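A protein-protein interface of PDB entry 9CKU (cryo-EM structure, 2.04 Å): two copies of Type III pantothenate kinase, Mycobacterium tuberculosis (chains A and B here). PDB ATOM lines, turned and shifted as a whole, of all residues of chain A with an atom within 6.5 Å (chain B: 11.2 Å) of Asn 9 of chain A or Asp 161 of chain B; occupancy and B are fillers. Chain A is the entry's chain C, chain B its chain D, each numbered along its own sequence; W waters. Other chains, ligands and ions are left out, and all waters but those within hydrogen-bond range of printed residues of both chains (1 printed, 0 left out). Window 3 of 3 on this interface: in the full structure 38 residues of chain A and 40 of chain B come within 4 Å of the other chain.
OG of Ser 134 of chain A lies within hydrogen-bond range of OD2 of Asp 161 of chain B (2.4 Å). The side-chain carboxylate of Asp 161 of chain B is in hydrogen-bond range of the side-chain hydroxyl of Ser 135 of chain A (2.6 Å). OG of Ser 159 of chain B lies close to OG of Ser 135 of chain A, 2.3 Å away.
OG1 of Thr 66 of chain A lies within hydrogen-bond range of OD1 of Asn 9 of chain A (3.1 Å). The backbone NH of Gly 155 of chain A lies within hydrogen-bond range of the backbone carbonyl oxygen of Ser 134 of chain A (3.4 Å). The backbone carbonyl oxygen (O) of Ile 136 of chain A is in hydrogen-bond range of the backbone NH (N) of Ala 153 of chain A. The side-chain hydroxyl (OG) of Ser 159 of chain B sits at hydrogen-bond distance from the side-chain carboxylate (OD1) of Asp 161 of chain B (2.5 Å).
Asn 9 of chain A touches Asp 161 of chain B. Ala 165 of chain B touches Asn 9 of chain A. O of Ile 152 of chain A touches CA of Met 190 of chain B, at 3.5 Å. Ile 152 of chain A touches Gly 193 of chain B. Ser 159 of chain B touches Ala 153 of chain A (OG to O, 3.5 Å). CA of Gly 193 of chain B touches CB of Ala 153 of chain A, 3.9 Å away. Pro 154 of chain A touches Gln 157 of chain B (CG to O, 3.4 Å). CA of Pro 154 of chain A touches OG of Ser 159 of chain B, at 3.8 Å. Phe 198 of chain B touches Pro 154 of chain A (CE2 to CG, 3.8 Å).
Printed residues of chain B within 4 Å of Asn 9 of chain A: Asp 161 and Ala 165. Of chain A, only Asn 9 (3.6 Å), Ser 134 (2.4 Å) and Ser 135 (2.6 Å) come within 4 Å of Asp 161 of chain B. No residue of chain B comes within 4 Å of Thr 34 of chain A. Of chain B, only Asp 161 (2.4 Å) comes within 4 Å of Ser 134 of chain A. Ser 135 of chain A touches two residues of chain B. Of the printed residues of chain B, Pro 154 of chain A touches Gln 157, Ser 159 and Phe 198. Of the printed residues of chain A, Gln 157 of chain B touches Pro 154. Of the printed residues of chain A, Phe 198 of chain B touches Pro 154 (3.8 Å). Of the printed residues of chain A, Gly 193 of chain B touches Ile 152 and Ala 153. The nearest residue of chain A that does not touch Asp 161 of chain B is Gly 155 of chain A (5.0 Å). The nearest printed residue of chain A that does not touch Gln 157 of chain B is Gln 157 of chain A (5.1 Å).
Of the 21 printed residues of chain B, 7 touch a printed residue of chain A. Printed residues of chain B that touch a printed residue of chain A: Gln 157, Ser 159, Asp 161, Ala 165, Met 190, Gly 193 and Phe 198. Printed residues of chain A that touch a printed residue of chain B: Asn 9, Ser 134, Ser 135, Ile 152, Ala 153 and Pro 154. Hydrophobic or aromatic side chains of chain A that line the printed part of chain B: Ala 153 and Pro 154.
1 position is printed for both chains.
Water W1 lies within hydrogen-bond range of the backbone carbonyl oxygen of Ile 152 of chain A (2.6 Å), the backbone carbonyl oxygen of Met 190 of chain B (2.7 Å) and the backbone NH of Ser 159 of chain B (2.9 Å).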
ATOM      1  N   VAL A   7     -28.317 -27.410  -0.765  1.00  0.00           N
ATOM      2  CA  VAL A   7     -29.106 -27.293   0.455  1.00  0.00           C
ATOM      3  C   VAL A   7     -28.815 -25.934   1.080  1.00  0.00           C
ATOM      4  O   VAL A   7     -27.666 -25.626   1.407  1.00  0.00           O
ATOM      5  CB  VAL A   7     -28.794 -28.432   1.444  1.00  0.00           C
ATOM      6  CG1 VAL A   7     -29.594 -28.263   2.728  1.00  0.00           C
ATOM      7  CG2 VAL A   7     -29.063 -29.792   0.818  1.00  0.00           C
ATOM      8  N   ARG A   8     -29.852 -25.126   1.240  1.00  0.00           N
ATOM      9  CA  ARG A   8     -29.796 -23.867   1.968  1.00  0.00           C
ATOM     10  C   ARG A   8     -30.557 -24.032   3.281  1.00  0.00           C
ATOM     11  O   ARG A   8     -31.152 -25.071   3.545  1.00  0.00           O
ATOM     12  CB  ARG A   8     -30.372 -22.725   1.131  1.00  0.00           C
ATOM     13  CG  ARG A   8     -29.862 -22.640  -0.290  1.00  0.00           C
ATOM     14  CD  ARG A   8     -28.372 -22.400  -0.372  1.00  0.00           C
ATOM     15  NE  ARG A   8     -27.979 -22.112  -1.747  1.00  0.00           N
ATOM     16  CZ  ARG A   8     -27.929 -20.903  -2.291  1.00  0.00           C
ATOM     17  NH1 ARG A   8     -28.133 -19.810  -1.578  1.00  0.00           N
ATOM     18  NH2 ARG A   8     -27.670 -20.790  -3.588  1.00  0.00           N
ATOM     19  N   ASN A   9     -30.550 -22.986   4.107  1.00  0.00           N
ATOM     20  CA  ASN A   9     -31.144 -23.095   5.439  1.00  0.00           C
ATOM     21  C   ASN A   9     -32.626 -23.459   5.374  1.00  0.00           C
ATOM     22  O   ASN A   9     -33.093 -24.305   6.141  1.00  0.00           O
ATOM     23  CB  ASN A   9     -30.953 -21.790   6.214  1.00  0.00           C
ATOM     24  CG  ASN A   9     -29.508 -21.561   6.626  1.00  0.00           C
ATOM     25  OD1 ASN A   9     -28.696 -22.477   6.617  1.00  0.00           O
ATOM     26  ND2 ASN A   9     -29.183 -20.331   6.983  1.00  0.00           N
ATOM     27  N   THR A  10     -33.378 -22.844   4.469  1.00  0.00           N
ATOM     28  CA  THR A  10     -34.821 -23.045   4.411  1.00  0.00           C
ATOM     29  C   THR A  10     -35.259 -23.968   3.278  1.00  0.00           C
ATOM     30  O   THR A  10     -36.221 -24.720   3.444  1.00  0.00           O
ATOM     31  CB  THR A  10     -35.539 -21.691   4.283  1.00  0.00           C
ATOM     32  OG1 THR A  10     -35.082 -20.810   5.315  1.00  0.00           O
ATOM     33  CG2 THR A  10     -37.033 -21.860   4.435  1.00  0.00           C
ATOM     34  N   HIS A  11     -34.584 -23.934   2.133  1.00  0.00           N
ATOM     35  CA  HIS A  11     -34.986 -24.720   0.977  1.00  0.00           C
ATOM     36  C   HIS A  11     -33.777 -25.369   0.326  1.00  0.00           C
ATOM     37  O   HIS A  11     -32.655 -24.870   0.403  1.00  0.00           O
ATOM     38  CB  HIS A  11     -35.731 -23.867  -0.061  1.00  0.00           C
ATOM     39  CG  HIS A  11     -37.114 -23.491   0.363  1.00  0.00           C
ATOM     40  ND1 HIS A  11     -37.385 -22.348   1.078  1.00  0.00           N
ATOM     41  CD2 HIS A  11     -38.295 -24.133   0.216  1.00  0.00           C
ATOM     42  CE1 HIS A  11     -38.679 -22.290   1.335  1.00  0.00           C
ATOM     43  NE2 HIS A  11     -39.254 -23.362   0.823  1.00  0.00           N
ATOM     44  N   ARG A  33     -38.337 -28.254   0.795  1.00  0.00           N
ATOM     45  CA  ARG A  33     -37.913 -27.687   2.068  1.00  0.00           C
ATOM     46  C   ARG A  33     -36.644 -28.368   2.560  1.00  0.00           C
ATOM     47  O   ARG A  33     -36.436 -29.564   2.357  1.00  0.00           O
ATOM     48  CB  ARG A  33     -38.998 -27.837   3.140  1.00  0.00           C
ATOM     49  CG  ARG A  33     -40.222 -26.970   2.947  1.00  0.00           C
ATOM     50  CD  ARG A  33     -41.487 -27.776   3.148  1.00  0.00           C
ATOM     51  NE  ARG A  33     -41.732 -28.150   4.531  1.00  0.00           N
ATOM     52  CZ  ARG A  33     -42.478 -29.182   4.906  1.00  0.00           C
ATOM     53  NH1 ARG A  33     -43.030 -29.998   4.024  1.00  0.00           N
ATOM     54  NH2 ARG A  33     -42.663 -29.408   6.202  1.00  0.00           N
ATOM     55  N   THR A  34     -35.792 -27.585   3.209  1.00  0.00           N
ATOM     56  CA  THR A  34     -34.666 -28.121   3.957  1.00  0.00           C
ATOM     57  C   THR A  34     -35.150 -28.445   5.365  1.00  0.00           C
ATOM     58  O   THR A  34     -35.684 -27.576   6.059  1.00  0.00           O
ATOM     59  CB  THR A  34     -33.497 -27.134   4.003  1.00  0.00           C
ATOM     60  OG1 THR A  34     -32.983 -26.916   2.684  1.00  0.00           O
ATOM     61  CG2 THR A  34     -32.389 -27.671   4.889  1.00  0.00           C
ATOM     62  N   GLU A  35     -34.983 -29.692   5.768  1.00  0.00           N
ATOM     63  CA  GLU A  35     -35.271 -30.143   7.122  1.00  0.00           C
ATOM     64  C   GLU A  35     -33.934 -30.507   7.753  1.00  0.00           C
ATOM     65  O   GLU A  35     -33.275 -31.456   7.322  1.00  0.00           O
ATOM     66  CB  GLU A  35     -36.242 -31.320   7.108  1.00  0.00           C
ATOM     67  CG  GLU A  35     -37.606 -30.972   6.542  1.00  0.00           C
ATOM     68  CD  GLU A  35     -38.504 -32.181   6.376  1.00  0.00           C
ATOM     69  OE1 GLU A  35     -38.197 -33.043   5.530  1.00  0.00           O
ATOM     70  OE2 GLU A  35     -39.515 -32.273   7.102  1.00  0.00           O
ATOM     71  N   SER A  36     -33.525 -29.736   8.758  1.00  0.00           N
ATOM     72  CA  SER A  36     -32.161 -29.853   9.257  1.00  0.00           C
ATOM     73  C   SER A  36     -31.894 -31.221   9.878  1.00  0.00           C
ATOM     74  O   SER A  36     -30.753 -31.687   9.870  1.00  0.00           O
ATOM     75  CB  SER A  36     -31.881 -28.740  10.265  1.00  0.00           C
ATOM     76  OG  SER A  36     -30.510 -28.696  10.594  1.00  0.00           O
ATOM     77  N   THR A  66     -25.361 -25.468   3.244  1.00  0.00           N
ATOM     78  CA  THR A  66     -25.122 -24.513   4.315  1.00  0.00           C
ATOM     79  C   THR A  66     -25.484 -25.080   5.682  1.00  0.00           C
ATOM     80  O   THR A  66     -25.300 -24.391   6.685  1.00  0.00           O
ATOM     81  CB  THR A  66     -25.916 -23.221   4.070  1.00  0.00           C
ATOM     82  OG1 THR A  66     -27.318 -23.506   4.072  1.00  0.00           O
ATOM     83  CG2 THR A  66     -25.523 -22.592   2.744  1.00  0.00           C
ATOM     84  N   VAL A  67     -25.989 -26.311   5.736  1.00  0.00           N
ATOM     85  CA  VAL A  67     -26.357 -26.990   6.975  1.00  0.00           C
ATOM     86  C   VAL A  67     -25.462 -28.217   7.146  1.00  0.00           C
ATOM     87  O   VAL A  67     -25.672 -29.223   6.456  1.00  0.00           O
ATOM     88  CB  VAL A  67     -27.845 -27.381   6.960  1.00  0.00           C
ATOM     89  CG1 VAL A  67     -28.262 -27.953   8.302  1.00  0.00           C
ATOM     90  CG2 VAL A  67     -28.705 -26.185   6.589  1.00  0.00           C
ATOM     91  N   GLY A 133     -32.122 -15.518  -1.116  1.00  0.00           N
ATOM     92  CA  GLY A 133     -32.494 -16.729  -0.423  1.00  0.00           C
ATOM     93  C   GLY A 133     -33.186 -16.412   0.886  1.00  0.00           C
ATOM     94  O   GLY A 133     -33.843 -15.384   1.036  1.00  0.00           O
ATOM     95  N   SER A 134     -33.027 -17.326   1.842  1.00  0.00           N
ATOM     96  CA  SER A 134     -33.434 -17.029   3.210  1.00  0.00           C
ATOM     97  C   SER A 134     -32.683 -15.814   3.746  1.00  0.00           C
ATOM     98  O   SER A 134     -33.163 -15.142   4.660  1.00  0.00           O
ATOM     99  CB  SER A 134     -33.196 -18.243   4.105  1.00  0.00           C
ATOM    100  OG  SER A 134     -31.825 -18.587   4.134  1.00  0.00           O
ATOM    101  N   SER A 135     -31.494 -15.548   3.212  1.00  0.00           N
ATOM    102  CA  SER A 135     -30.810 -14.274   3.361  1.00  0.00           C
ATOM    103  C   SER A 135     -30.523 -13.715   1.978  1.00  0.00           C
ATOM    104  O   SER A 135     -30.487 -14.447   0.989  1.00  0.00           O
ATOM    105  CB  SER A 135     -29.483 -14.406   4.122  1.00  0.00           C
ATOM    106  OG  SER A 135     -29.686 -14.755   5.475  1.00  0.00           O
ATOM    107  N   ILE A 136     -30.322 -12.406   1.909  1.00  0.00           N
ATOM    108  CA  ILE A 136     -29.789 -11.782   0.707  1.00  0.00           C
ATOM    109  C   ILE A 136     -28.277 -11.712   0.858  1.00  0.00           C
ATOM    110  O   ILE A 136     -27.771 -11.099   1.799  1.00  0.00           O
ATOM    111  CB  ILE A 136     -30.386 -10.388   0.473  1.00  0.00           C
ATOM    112  CG1 ILE A 136     -31.870 -10.507   0.129  1.00  0.00           C
ATOM    113  CG2 ILE A 136     -29.619  -9.678  -0.639  1.00  0.00           C
ATOM    114  CD1 ILE A 136     -32.612  -9.201   0.102  1.00  0.00           C
ATOM    115  N   ILE A 152     -24.240  -9.745   4.042  1.00  0.00           N
ATOM    116  CA  ILE A 152     -25.333 -10.678   4.274  1.00  0.00           C
ATOM    117  C   ILE A 152     -26.433  -9.918   4.997  1.00  0.00           C
ATOM    118  O   ILE A 152     -26.217  -9.423   6.108  1.00  0.00           O
ATOM    119  CB  ILE A 152     -24.879 -11.899   5.094  1.00  0.00           C
ATOM    120  CG1 ILE A 152     -23.736 -12.631   4.375  1.00  0.00           C
ATOM    121  CG2 ILE A 152     -26.050 -12.835   5.358  1.00  0.00           C
ATOM    122  CD1 ILE A 152     -23.074 -13.720   5.198  1.00  0.00           C
ATOM    123  N   ALA A 153     -27.599  -9.827   4.376  1.00  0.00           N
ATOM    124  CA  ALA A 153     -28.732  -9.076   4.880  1.00  0.00           C
ATOM    125  C   ALA A 153     -29.947  -9.981   5.027  1.00  0.00           C
ATOM    126  O   ALA A 153     -29.984 -11.080   4.465  1.00  0.00           O
ATOM    127  CB  ALA A 153     -29.070  -7.907   3.941  1.00  0.00           C
ATOM    128  N   PRO A 154     -30.956  -9.557   5.786  1.00  0.00           N
ATOM    129  CA  PRO A 154     -32.178 -10.361   5.904  1.00  0.00           C
ATOM    130  C   PRO A 154     -32.837 -10.589   4.550  1.00  0.00           C
ATOM    131  O   PRO A 154     -32.812  -9.733   3.666  1.00  0.00           O
ATOM    132  CB  PRO A 154     -33.075  -9.519   6.821  1.00  0.00           C
ATOM    133  CG  PRO A 154     -32.164  -8.607   7.530  1.00  0.00           C
ATOM    134  CD  PRO A 154     -31.014  -8.347   6.625  1.00  0.00           C
ATOM    135  N   GLY A 155     -33.416 -11.769   4.397  1.00  0.00           N
ATOM    136  CA  GLY A 155     -34.124 -12.088   3.178  1.00  0.00           C
ATOM    137  C   GLY A 155     -35.362 -11.231   2.989  1.00  0.00           C
ATOM    138  O   GLY A 155     -35.855 -10.581   3.906  1.00  0.00           O
ATOM    139  N   GLN A 157     -38.909 -10.061   2.913  1.00  0.00           N
ATOM    140  CA  GLN A 157     -40.032 -10.455   3.753  1.00  0.00           C
ATOM    141  C   GLN A 157     -40.806  -9.238   4.247  1.00  0.00           C
ATOM    142  O   GLN A 157     -40.263  -8.137   4.346  1.00  0.00           O
ATOM    143  CB  GLN A 157     -39.505 -11.211   4.980  1.00  0.00           C
ATOM    144  CG  GLN A 157     -38.582 -10.306   5.825  1.00  0.00           C
ATOM    145  CD  GLN A 157     -37.787 -11.035   6.890  1.00  0.00           C
ATOM    146  OE1 GLN A 157     -38.306 -11.350   7.957  1.00  0.00           O
ATOM    147  NE2 GLN A 157     -36.512 -11.274   6.615  1.00  0.00           N
ATOM    148  N   GLN B 157     -32.297  -5.128  11.486  1.00  0.00           N
ATOM    149  CA  GLN B 157     -31.855  -6.348  12.138  1.00  0.00           C
ATOM    150  C   GLN B 157     -30.853  -7.087  11.265  1.00  0.00           C
ATOM    151  O   GLN B 157     -30.779  -6.865  10.057  1.00  0.00           O
ATOM    152  CB  GLN B 157     -33.068  -7.252  12.382  1.00  0.00           C
ATOM    153  CG  GLN B 157     -33.792  -7.582  11.062  1.00  0.00           C
ATOM    154  CD  GLN B 157     -35.140  -8.243  11.244  1.00  0.00           C
ATOM    155  OE1 GLN B 157     -35.232  -9.442  11.485  1.00  0.00           O
ATOM    156  NE2 GLN B 157     -36.202  -7.454  11.117  1.00  0.00           N
ATOM    157  N   VAL B 158     -30.088  -7.972  11.903  1.00  0.00           N
ATOM    158  CA  VAL B 158     -29.173  -8.846  11.178  1.00  0.00           C
ATOM    159  C   VAL B 158     -29.991  -9.995  10.601  1.00  0.00           C
ATOM    160  O   VAL B 158     -31.100 -10.276  11.054  1.00  0.00           O
ATOM    161  CB  VAL B 158     -28.018  -9.361  12.063  1.00  0.00           C
ATOM    162  CG1 VAL B 158     -27.142  -8.209  12.520  1.00  0.00           C
ATOM    163  CG2 VAL B 158     -28.541 -10.172  13.254  1.00  0.00           C
ATOM    164  N   SER B 159     -29.458 -10.664   9.589  1.00  0.00           N
ATOM    165  CA  SER B 159     -30.234 -11.742   8.994  1.00  0.00           C
ATOM    166  C   SER B 159     -30.529 -12.809  10.042  1.00  0.00           C
ATOM    167  O   SER B 159     -29.621 -13.316  10.703  1.00  0.00           O
ATOM    168  CB  SER B 159     -29.468 -12.347   7.822  1.00  0.00           C
ATOM    169  OG  SER B 159     -30.250 -13.325   7.167  1.00  0.00           O
ATOM    170  N   SER B 160     -31.820 -13.132  10.184  1.00  0.00           N
ATOM    171  CA  SER B 160     -32.260 -14.095  11.189  1.00  0.00           C
ATOM    172  C   SER B 160     -31.730 -15.489  10.905  1.00  0.00           C
ATOM    173  O   SER B 160     -31.241 -16.168  11.812  1.00  0.00           O
ATOM    174  CB  SER B 160     -33.787 -14.118  11.264  1.00  0.00           C
ATOM    175  OG  SER B 160     -34.284 -13.023  12.009  1.00  0.00           O
ATOM    176  N   ASP B 161     -31.816 -15.940   9.654  1.00  0.00           N
ATOM    177  CA  ASP B 161     -31.315 -17.275   9.350  1.00  0.00           C
ATOM    178  C   ASP B 161     -29.807 -17.345   9.539  1.00  0.00           C
ATOM    179  O   ASP B 161     -29.287 -18.362  10.003  1.00  0.00           O
ATOM    180  CB  ASP B 161     -31.693 -17.706   7.932  1.00  0.00           C
ATOM    181  CG  ASP B 161     -31.428 -16.647   6.905  1.00  0.00           C
ATOM    182  OD1 ASP B 161     -31.634 -15.452   7.201  1.00  0.00           O
ATOM    183  OD2 ASP B 161     -30.972 -17.020   5.808  1.00  0.00           O
ATOM    184  N   ALA B 162     -29.085 -16.279   9.183  1.00  0.00           N
ATOM    185  CA  ALA B 162     -27.644 -16.273   9.407  1.00  0.00           C
ATOM    186  C   ALA B 162     -27.322 -16.340  10.894  1.00  0.00           C
ATOM    187  O   ALA B 162     -26.455 -17.114  11.320  1.00  0.00           O
ATOM    188  CB  ALA B 162     -27.014 -15.032   8.778  1.00  0.00           C
ATOM    189  N   ALA B 163     -28.026 -15.548  11.705  1.00  0.00           N
ATOM    190  CA  ALA B 163     -27.797 -15.579  13.144  1.00  0.00           C
ATOM    191  C   ALA B 163     -28.102 -16.956  13.717  1.00  0.00           C
ATOM    192  O   ALA B 163     -27.322 -17.495  14.510  1.00  0.00           O
ATOM    193  CB  ALA B 163     -28.648 -14.511  13.831  1.00  0.00           C
ATOM    194  N   ALA B 164     -29.226 -17.550  13.309  1.00  0.00           N
ATOM    195  CA  ALA B 164     -29.599 -18.867  13.810  1.00  0.00           C
ATOM    196  C   ALA B 164     -28.595 -19.932  13.389  1.00  0.00           C
ATOM    197  O   ALA B 164     -28.260 -20.814  14.186  1.00  0.00           O
ATOM    198  CB  ALA B 164     -30.998 -19.232  13.321  1.00  0.00           C
ATOM    199  N   ALA B 165     -28.108 -19.870  12.150  1.00  0.00           N
ATOM    200  CA  ALA B 165     -27.126 -20.832  11.672  1.00  0.00           C
ATOM    201  C   ALA B 165     -25.755 -20.634  12.301  1.00  0.00           C
ATOM    202  O   ALA B 165     -24.941 -21.560  12.278  1.00  0.00           O
ATOM    203  CB  ALA B 165     -27.007 -20.739  10.152  1.00  0.00           C
ATOM    204  N   ARG B 166     -25.481 -19.451  12.854  1.00  0.00           N
ATOM    205  CA  ARG B 166     -24.178 -19.222  13.474  1.00  0.00           C
ATOM    206  C   ARG B 166     -23.915 -20.210  14.610  1.00  0.00           C
ATOM    207  O   ARG B 166     -22.767 -20.608  14.836  1.00  0.00           O
ATOM    208  CB  ARG B 166     -24.085 -17.781  13.976  1.00  0.00           C
ATOM    209  CG  ARG B 166     -22.839 -17.042  13.504  1.00  0.00           C
ATOM    210  CD  ARG B 166     -22.609 -15.763  14.299  1.00  0.00           C
ATOM    211  NE  ARG B 166     -21.192 -15.541  14.554  1.00  0.00           N
ATOM    212  CZ  ARG B 166     -20.709 -14.768  15.518  1.00  0.00           C
ATOM    213  NH1 ARG B 166     -21.505 -14.092  16.331  1.00  0.00           N
ATOM    214  NH2 ARG B 166     -19.392 -14.674  15.674  1.00  0.00           N
ATOM    215  N   SER B 167     -24.968 -20.618  15.329  1.00  0.00           N
ATOM    216  CA  SER B 167     -24.898 -21.604  16.411  1.00  0.00           C
ATOM    217  C   SER B 167     -24.540 -20.959  17.745  1.00  0.00           C
ATOM    218  O   SER B 167     -24.199 -19.774  17.801  1.00  0.00           O
ATOM    219  CB  SER B 167     -23.895 -22.718  16.103  1.00  0.00           C
ATOM    220  OG  SER B 167     -22.599 -22.371  16.544  1.00  0.00           O
ATOM    221  N   ALA B 168     -24.637 -21.739  18.829  1.00  0.00           N
ATOM    222  CA  ALA B 168     -24.479 -21.213  20.181  1.00  0.00           C
ATOM    223  C   ALA B 168     -23.024 -21.057  20.611  1.00  0.00           C
ATOM    224  O   ALA B 168     -22.768 -20.384  21.615  1.00  0.00           O
ATOM    225  CB  ALA B 168     -25.203 -22.123  21.176  1.00  0.00           C
ATOM    226  N   LEU B 170     -20.643 -19.472  19.038  1.00  0.00           N
ATOM    227  CA  LEU B 170     -20.002 -18.298  18.455  1.00  0.00           C
ATOM    228  C   LEU B 170     -20.527 -16.973  18.992  1.00  0.00           C
ATOM    229  O   LEU B 170     -19.902 -15.940  18.735  1.00  0.00           O
ATOM    230  CB  LEU B 170     -20.171 -18.303  16.931  1.00  0.00           C
ATOM    231  CG  LEU B 170     -19.437 -19.399  16.162  1.00  0.00           C
ATOM    232  CD1 LEU B 170     -19.793 -19.336  14.689  1.00  0.00           C
ATOM    233  CD2 LEU B 170     -17.931 -19.274  16.353  1.00  0.00           C
ATOM    234  N   ARG B 171     -21.651 -16.971  19.710  1.00  0.00           N
ATOM    235  CA  ARG B 171     -22.206 -15.752  20.292  1.00  0.00           C
ATOM    236  C   ARG B 171     -22.891 -14.887  19.238  1.00  0.00           C
ATOM    237  O   ARG B 171     -22.617 -15.017  18.040  1.00  0.00           O
ATOM    238  CB  ARG B 171     -21.116 -14.944  21.000  1.00  0.00           C
ATOM    239  CG  ARG B 171     -21.614 -14.110  22.162  1.00  0.00           C
ATOM    240  CD  ARG B 171     -20.501 -13.260  22.729  1.00  0.00           C
ATOM    241  NE  ARG B 171     -20.098 -12.219  21.792  1.00  0.00           N
ATOM    242  CZ  ARG B 171     -19.193 -11.284  22.049  1.00  0.00           C
ATOM    243  NH1 ARG B 171     -18.561 -11.232  23.211  1.00  0.00           N
ATOM    244  NH2 ARG B 171     -18.915 -10.379  21.116  1.00  0.00           N
ATOM    245  N   ARG B 172     -23.774 -13.997  19.679  1.00  0.00           N
ATOM    246  CA  ARG B 172     -24.624 -13.244  18.769  1.00  0.00           C
ATOM    247  C   ARG B 172     -23.865 -12.077  18.151  1.00  0.00           C
ATOM    248  O   ARG B 172     -22.913 -11.547  18.729  1.00  0.00           O
ATOM    249  CB  ARG B 172     -25.861 -12.725  19.501  1.00  0.00           C
ATOM    250  CG  ARG B 172     -25.563 -11.639  20.523  1.00  0.00           C
ATOM    251  CD  ARG B 172     -26.749 -11.394  21.450  1.00  0.00           C
ATOM    252  NE  ARG B 172     -27.041 -12.552  22.290  1.00  0.00           N
ATOM    253  CZ  ARG B 172     -27.764 -12.514  23.403  1.00  0.00           C
ATOM    254  NH1 ARG B 172     -28.274 -11.382  23.860  1.00  0.00           N
ATOM    255  NH2 ARG B 172     -27.962 -13.638  24.085  1.00  0.00           N
ATOM    256  N   VAL B 173     -24.309 -11.669  16.966  1.00  0.00           N
ATOM    257  CA  VAL B 173     -23.705 -10.536  16.278  1.00  0.00           C
ATOM    258  C   VAL B 173     -24.383  -9.252  16.725  1.00  0.00           C
ATOM    259  O   VAL B 173     -25.609  -9.117  16.660  1.00  0.00           O
ATOM    260  CB  VAL B 173     -23.797 -10.713  14.748  1.00  0.00           C
ATOM    261  CG1 VAL B 173     -23.523  -9.462  13.893  1.00  0.00           C
ATOM    262  CG2 VAL B 173     -23.547 -12.141  14.200  1.00  0.00           C
ATOM    263  N   THR B 186     -17.677 -13.248   8.976  1.00  0.00           N
ATOM    264  CA  THR B 186     -19.129 -13.381   9.034  1.00  0.00           C
ATOM    265  C   THR B 186     -19.780 -12.223   9.779  1.00  0.00           C
ATOM    266  O   THR B 186     -20.815 -11.707   9.345  1.00  0.00           O
ATOM    267  CB  THR B 186     -19.508 -14.709   9.687  1.00  0.00           C
ATOM    268  OG1 THR B 186     -19.020 -15.788   8.888  1.00  0.00           O
ATOM    269  CG2 THR B 186     -21.022 -14.837   9.823  1.00  0.00           C
ATOM    270  N   MET B 190     -22.521  -9.653   8.145  1.00  0.00           N
ATOM    271  CA  MET B 190     -23.872  -9.484   8.670  1.00  0.00           C
ATOM    272  C   MET B 190     -24.117  -8.041   9.105  1.00  0.00           C
ATOM    273  O   MET B 190     -25.203  -7.496   8.885  1.00  0.00           O
ATOM    274  CB  MET B 190     -24.110 -10.462   9.820  1.00  0.00           C
ATOM    275  CG  MET B 190     -24.200 -11.924   9.380  1.00  0.00           C
ATOM    276  SD  MET B 190     -24.091 -13.131  10.717  1.00  0.00           S
ATOM    277  CE  MET B 190     -25.650 -12.890  11.552  1.00  0.00           C
ATOM    278  N   GLY B 193     -24.581  -5.944   5.892  1.00  0.00           N
ATOM    279  CA  GLY B 193     -25.939  -6.182   5.465  1.00  0.00           C
ATOM    280  C   GLY B 193     -26.910  -5.349   6.268  1.00  0.00           C
ATOM    281  O   GLY B 193     -27.522  -4.444   5.720  1.00  0.00           O
ATOM    282  N   ALA B 194     -26.952  -5.534   7.584  1.00  0.00           N
ATOM    283  CA  ALA B 194     -27.917  -4.801   8.395  1.00  0.00           C
ATOM    284  C   ALA B 194     -27.803  -3.291   8.177  1.00  0.00           C
ATOM    285  O   ALA B 194     -28.717  -2.661   7.635  1.00  0.00           O
ATOM    286  CB  ALA B 194     -27.732  -5.156   9.868  1.00  0.00           C
ATOM    287  N   PHE B 198     -30.185  -1.542   5.331  1.00  0.00           N
ATOM    288  CA  PHE B 198     -31.380  -0.847   5.786  1.00  0.00           C
ATOM    289  C   PHE B 198     -31.284   0.652   5.535  1.00  0.00           C
ATOM    290  O   PHE B 198     -32.313   1.296   5.305  1.00  0.00           O
ATOM    291  CB  PHE B 198     -31.652  -1.158   7.255  1.00  0.00           C
ATOM    292  CG  PHE B 198     -32.402  -2.441   7.450  1.00  0.00           C
ATOM    293  CD1 PHE B 198     -33.782  -2.470   7.375  1.00  0.00           C
ATOM    294  CD2 PHE B 198     -31.725  -3.625   7.688  1.00  0.00           C
ATOM    295  CE1 PHE B 198     -34.471  -3.651   7.540  1.00  0.00           C
ATOM    296  CE2 PHE B 198     -32.411  -4.807   7.858  1.00  0.00           C
ATOM    297  CZ  PHE B 198     -33.784  -4.819   7.784  1.00  0.00           C
HETATM  298  O   HOH W   1     -27.450  -8.939   8.331  1.00  0.00           O
